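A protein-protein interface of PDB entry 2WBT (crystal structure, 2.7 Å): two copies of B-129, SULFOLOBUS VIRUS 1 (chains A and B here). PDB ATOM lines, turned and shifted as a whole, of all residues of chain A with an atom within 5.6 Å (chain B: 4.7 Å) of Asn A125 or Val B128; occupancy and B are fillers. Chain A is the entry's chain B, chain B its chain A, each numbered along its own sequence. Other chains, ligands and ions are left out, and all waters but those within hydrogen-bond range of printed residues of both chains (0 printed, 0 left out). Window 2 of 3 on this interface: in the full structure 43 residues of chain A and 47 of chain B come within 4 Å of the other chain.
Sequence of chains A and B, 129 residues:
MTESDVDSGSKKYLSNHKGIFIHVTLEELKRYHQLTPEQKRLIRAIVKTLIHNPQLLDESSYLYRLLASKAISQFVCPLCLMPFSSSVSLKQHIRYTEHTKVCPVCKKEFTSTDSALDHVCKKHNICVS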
ATOM      1  N   VAL A 120     -26.749 -30.784 -13.908  1.00  0.00           N
ATOM      2  CA  VAL A 120     -26.206 -30.181 -15.136  1.00  0.00           C
ATOM      3  C   VAL A 120     -25.774 -28.726 -14.913  1.00  0.00           C
ATOM      4  O   VAL A 120     -24.777 -28.271 -15.470  1.00  0.00           O
ATOM      5  CB  VAL A 120     -27.222 -30.239 -16.307  1.00  0.00           C
ATOM      6  CG1 VAL A 120     -26.590 -29.707 -17.588  1.00  0.00           C
ATOM      7  CG2 VAL A 120     -27.707 -31.667 -16.529  1.00  0.00           C
ATOM      8  N   CYS A 121     -26.539 -28.007 -14.097  1.00  0.00           N
ATOM      9  CA  CYS A 121     -26.202 -26.635 -13.704  1.00  0.00           C
ATOM     10  C   CYS A 121     -24.986 -26.603 -12.780  1.00  0.00           C
ATOM     11  O   CYS A 121     -24.002 -25.912 -13.052  1.00  0.00           O
ATOM     12  CB  CYS A 121     -27.400 -25.995 -12.993  1.00  0.00           C
ATOM     13  SG  CYS A 121     -27.173 -24.286 -12.408  1.00  0.00           S
ATOM     14  N   LYS A 122     -25.072 -27.362 -11.692  1.00  0.00           N
ATOM     15  CA  LYS A 122     -24.037 -27.385 -10.651  1.00  0.00           C
ATOM     16  C   LYS A 122     -22.686 -27.910 -11.130  1.00  0.00           C
ATOM     17  O   LYS A 122     -21.654 -27.277 -10.904  1.00  0.00           O
ATOM     18  CB  LYS A 122     -24.501 -28.226  -9.453  1.00  0.00           C
ATOM     19  CG  LYS A 122     -24.916 -27.413  -8.239  1.00  0.00           C
ATOM     20  CD  LYS A 122     -25.869 -28.203  -7.358  1.00  0.00           C
ATOM     21  CE  LYS A 122     -26.087 -27.528  -6.013  1.00  0.00           C
ATOM     22  NZ  LYS A 122     -27.149 -26.482  -6.077  1.00  0.00           N
ATOM     23  N   LYS A 123     -22.702 -29.066 -11.786  1.00  0.00           N
ATOM     24  CA  LYS A 123     -21.468 -29.759 -12.166  1.00  0.00           C
ATOM     25  C   LYS A 123     -20.928 -29.347 -13.520  1.00  0.00           C
ATOM     26  O   LYS A 123     -19.719 -29.392 -13.753  1.00  0.00           O
ATOM     27  CB  LYS A 123     -21.691 -31.272 -12.161  1.00  0.00           C
ATOM     28  CG  LYS A 123     -22.038 -31.831 -10.796  1.00  0.00           C
ATOM     29  CD  LYS A 123     -20.941 -31.542  -9.780  1.00  0.00           C
ATOM     30  CE  LYS A 123     -21.309 -32.057  -8.408  1.00  0.00           C
ATOM     31  NZ  LYS A 123     -22.349 -31.211  -7.754  1.00  0.00           N
ATOM     32  N   HIS A 124     -21.827 -28.946 -14.408  1.00  0.00           N
ATOM     33  CA  HIS A 124     -21.454 -28.684 -15.798  1.00  0.00           C
ATOM     34  C   HIS A 124     -21.617 -27.230 -16.246  1.00  0.00           C
ATOM     35  O   HIS A 124     -21.209 -26.888 -17.348  1.00  0.00           O
ATOM     36  CB  HIS A 124     -22.224 -29.615 -16.733  1.00  0.00           C
ATOM     37  CG  HIS A 124     -21.985 -31.066 -16.462  1.00  0.00           C
ATOM     38  ND1 HIS A 124     -20.859 -31.730 -16.900  1.00  0.00           N
ATOM     39  CD2 HIS A 124     -22.724 -31.980 -15.788  1.00  0.00           C
ATOM     40  CE1 HIS A 124     -20.917 -32.991 -16.511  1.00  0.00           C
ATOM     41  NE2 HIS A 124     -22.038 -33.169 -15.836  1.00  0.00           N
ATOM     42  N   ASN A 125     -22.213 -26.381 -15.411  1.00  0.00           N
ATOM     43  CA  ASN A 125     -22.313 -24.932 -15.683  1.00  0.00           C
ATOM     44  C   ASN A 125     -23.454 -24.528 -16.627  1.00  0.00           C
ATOM     45  O   ASN A 125     -23.525 -23.376 -17.060  1.00  0.00           O
ATOM     46  CB  ASN A 125     -20.984 -24.363 -16.221  1.00  0.00           C
ATOM     47  CG  ASN A 125     -19.843 -24.493 -15.229  1.00  0.00           C
ATOM     48  OD1 ASN A 125     -18.680 -24.596 -15.625  1.00  0.00           O
ATOM     49  ND2 ASN A 125     -20.165 -24.470 -13.938  1.00  0.00           N
ATOM     50  N   ILE A 126     -24.346 -25.467 -16.928  1.00  0.00           N
ATOM     51  CA  ILE A 126     -25.464 -25.213 -17.837  1.00  0.00           C
ATOM     52  C   ILE A 126     -26.747 -25.013 -17.039  1.00  0.00           C
ATOM     53  O   ILE A 126     -27.376 -25.974 -16.592  1.00  0.00           O
ATOM     54  CB  ILE A 126     -25.647 -26.363 -18.842  1.00  0.00           C
ATOM     55  CG1 ILE A 126     -24.337 -26.647 -19.582  1.00  0.00           C
ATOM     56  CG2 ILE A 126     -26.749 -26.030 -19.838  1.00  0.00           C
ATOM     57  CD1 ILE A 126     -23.755 -25.458 -20.307  1.00  0.00           C
ATOM     58  N   CYS A 127     -27.129 -23.750 -16.884  1.00  0.00           N
ATOM     59  CA  CYS A 127     -28.247 -23.364 -16.034  1.00  0.00           C
ATOM     60  C   CYS A 127     -29.266 -22.582 -16.856  1.00  0.00           C
ATOM     61  O   CYS A 127     -28.913 -21.938 -17.847  1.00  0.00           O
ATOM     62  CB  CYS A 127     -27.740 -22.531 -14.854  1.00  0.00           C
ATOM     63  SG  CYS A 127     -26.337 -23.291 -13.973  1.00  0.00           S
ATOM     64  N   LYS B  70     -12.136 -28.114 -17.149  1.00  0.00           N
ATOM     65  CA  LYS B  70     -13.166 -28.854 -16.411  1.00  0.00           C
ATOM     66  C   LYS B  70     -12.715 -30.251 -15.969  1.00  0.00           C
ATOM     67  O   LYS B  70     -13.216 -30.784 -14.978  1.00  0.00           O
ATOM     68  CB  LYS B  70     -14.464 -28.949 -17.224  1.00  0.00           C
ATOM     69  CG  LYS B  70     -15.487 -27.900 -16.840  1.00  0.00           C
ATOM     70  CD  LYS B  70     -16.115 -28.230 -15.491  1.00  0.00           C
ATOM     71  CE  LYS B  70     -17.019 -27.121 -15.018  1.00  0.00           C
ATOM     72  NZ  LYS B  70     -18.135 -26.925 -15.982  1.00  0.00           N
ATOM     73  N   VAL B  76     -14.282 -23.798 -12.469  1.00  0.00           N
ATOM     74  CA  VAL B  76     -13.593 -23.083 -13.539  1.00  0.00           C
ATOM     75  C   VAL B  76     -14.248 -21.725 -13.771  1.00  0.00           C
ATOM     76  O   VAL B  76     -15.459 -21.567 -13.610  1.00  0.00           O
ATOM     77  CB  VAL B  76     -13.628 -23.882 -14.861  1.00  0.00           C
ATOM     78  CG1 VAL B  76     -12.765 -23.209 -15.921  1.00  0.00           C
ATOM     79  CG2 VAL B  76     -13.165 -25.314 -14.631  1.00  0.00           C
ATOM     80  N   PRO B  78     -15.457 -18.854 -16.287  1.00  0.00           N
ATOM     81  CA  PRO B  78     -15.850 -18.775 -17.694  1.00  0.00           C
ATOM     82  C   PRO B  78     -15.020 -17.782 -18.507  1.00  0.00           C
ATOM     83  O   PRO B  78     -14.776 -18.017 -19.689  1.00  0.00           O
ATOM     84  CB  PRO B  78     -17.314 -18.319 -17.627  1.00  0.00           C
ATOM     85  CG  PRO B  78     -17.750 -18.602 -16.233  1.00  0.00           C
ATOM     86  CD  PRO B  78     -16.538 -18.391 -15.402  1.00  0.00           C
ATOM     87  N   ILE B  94     -13.099 -14.439  -8.982  1.00  0.00           N
ATOM     88  CA  ILE B  94     -14.095 -13.690  -9.746  1.00  0.00           C
ATOM     89  C   ILE B  94     -14.380 -12.336  -9.102  1.00  0.00           C
ATOM     90  O   ILE B  94     -14.476 -11.323  -9.797  1.00  0.00           O
ATOM     91  CB  ILE B  94     -15.408 -14.488  -9.902  1.00  0.00           C
ATOM     92  CG1 ILE B  94     -15.238 -15.574 -10.964  1.00  0.00           C
ATOM     93  CG2 ILE B  94     -16.560 -13.571 -10.297  1.00  0.00           C
ATOM     94  CD1 ILE B  94     -16.411 -16.527 -11.056  1.00  0.00           C
ATOM     95  N   ASN B 125     -24.567 -19.662 -22.226  1.00  0.00           N
ATOM     96  CA  ASN B 125     -25.038 -20.664 -21.285  1.00  0.00           C
ATOM     97  C   ASN B 125     -23.946 -21.325 -20.459  1.00  0.00           C
ATOM     98  O   ASN B 125     -24.066 -22.489 -20.080  1.00  0.00           O
ATOM     99  CB  ASN B 125     -25.859 -21.727 -22.011  1.00  0.00           C
ATOM    100  CG  ASN B 125     -27.136 -22.063 -21.280  1.00  0.00           C
ATOM    101  OD1 ASN B 125     -28.191 -22.211 -21.896  1.00  0.00           O
ATOM    102  ND2 ASN B 125     -27.055 -22.179 -19.958  1.00  0.00           N
ATOM    103  N   ILE B 126     -22.892 -20.576 -20.166  1.00  0.00           N
ATOM    104  CA  ILE B 126     -21.840 -21.066 -19.288  1.00  0.00           C
ATOM    105  C   ILE B 126     -21.856 -20.205 -18.035  1.00  0.00           C
ATOM    106  O   ILE B 126     -21.482 -19.032 -18.063  1.00  0.00           O
ATOM    107  CB  ILE B 126     -20.478 -21.058 -19.984  1.00  0.00           C
ATOM    108  CG1 ILE B 126     -20.526 -21.998 -21.192  1.00  0.00           C
ATOM    109  CG2 ILE B 126     -19.379 -21.483 -19.016  1.00  0.00           C
ATOM    110  CD1 ILE B 126     -19.199 -22.184 -21.881  1.00  0.00           C
ATOM    111  N   CYS B 127     -22.299 -20.815 -16.940  1.00  0.00           N
ATOM    112  CA  CYS B 127     -22.741 -20.087 -15.760  1.00  0.00           C
ATOM    113  C   CYS B 127     -22.059 -20.598 -14.497  1.00  0.00           C
ATOM    114  O   CYS B 127     -21.777 -21.792 -14.373  1.00  0.00           O
ATOM    115  CB  CYS B 127     -24.259 -20.227 -15.620  1.00  0.00           C
ATOM    116  SG  CYS B 127     -25.187 -19.779 -17.113  1.00  0.00           S
ATOM    117  N   VAL B 128     -21.796 -19.684 -13.564  1.00  0.00           N
ATOM    118  CA  VAL B 128     -21.212 -20.033 -12.269  1.00  0.00           C
ATOM    119  C   VAL B 128     -21.830 -19.213 -11.138  1.00  0.00           C
ATOM    120  O   VAL B 128     -22.220 -18.060 -11.332  1.00  0.00           O
ATOM    121  CB  VAL B 128     -19.677 -19.828 -12.251  1.00  0.00           C
ATOM    122  CG1 VAL B 128     -19.002 -20.731 -13.273  1.00  0.00           C
ATOM    123  CG2 VAL B 128     -19.324 -18.367 -12.505  1.00  0.00           C
ATOM    124  N   SER B 129     -21.922 -19.829  -9.963  1.00  0.00           N
ATOM    125  CA  SER B 129     -22.338 -19.140  -8.740  1.00  0.00           C
ATOM    126  C   SER B 129     -21.394 -17.985  -8.413  1.00  0.00           C
ATOM    127  O   SER B 129     -21.785 -16.818  -8.465  1.00  0.00           O
ATOM    128  CB  SER B 129     -22.372 -20.118  -7.563  1.00  0.00           C
ATOM    129  OG  SER B 129     -23.489 -20.985  -7.654  1.00  0.00           O
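NZ of Lys B70 is in hydrogen-bond range of O of His A124 (3.4 Å). OD1 of Asn A125 is in hydrogen-bond range of NZ of Lys B70 (2.4 Å). The side-chain amide nitrogen of Asn B125 lies within hydrogen-bond range of the backbone carbonyl oxygen of Cys A127, at 2.8 Å. The backbone carbonyl oxygen of Asn A125 sits at hydrogen-bond distance from the backbone NH of Cys B127, at 2.8 Å. The backbone carbonyl oxygen (O) of Asn B125 sits close to the backbone carbonyl oxygen (O) of Asn A125.
O of Val A120 is in hydrogen-bond range of N of Asn A125 (3.2 Å). The backbone NH (N) of Ile A126 is in hydrogen-bond range of the backbone carbonyl oxygen (O) of Val A120. The backbone carbonyl oxygen of Ile A126 lies close to the backbone NH of Cys A121 (3.3 Å). The side-chain sulfur of Cys A121 is disulfide-bonded to the side-chain sulfur of Cys A127.
Among the printed residues, merely in contact across the chains: Lys A123 with Lys B70 (3.7 Å), Asn A125 with Ile B126 (3.6 Å), Asn A125 with Val B128 (3.97 Å) and Ile A126 with Asn B125 (3.0 Å).
Of chain B, only Lys B70, Asn B125, Ile B126, Cys B127 and Val B128 come within 4 Å of Asn A125. Of the printed residues of chain B, Cys A127 touches Asn B125. Printed residues of chain A within 4 Å of Lys B70: Lys A123, His A124 and Asn A125. Pro B78 touches none of the printed residues of chain A. Of the printed residues of chain A, Ile B126 touches Asn A125 (3.6 Å). Printed residues of chain A within 4 Å of Cys B127: Asn A125. Val B128 touches just one residue of chain A: Asn A125 (3.97 Å). Ser B129 touches none of the printed residues of chain A. The nearest printed residue of chain B that does not touch Asn A125 is Val B76 (4.9 Å). The nearest printed residue of chain A that does not touch Val B128 is Cys A127 (5.8 Å).
Hydrophobic or aromatic side chains of chain A that line the printed part of chain B: Ile A126. Printed residues of chain B that touch a printed residue of chain A: Lys B70, Asn B125, Ile B126, Cys B127 and Val B128.
Asn A125 touches its own counterpart, Asn B125. Asn A125 touches Ile B126, and with the chains exchanged Ile A126 touches Asn B125. Asn A125 touches Cys B127, and with the chains exchanged Cys A127 touches Asn B125. 3 positions are printed for both chains. Of the 9 pairs that touch across the chains among the printed residues, 5 have their exchanged pair printed and touching as well.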
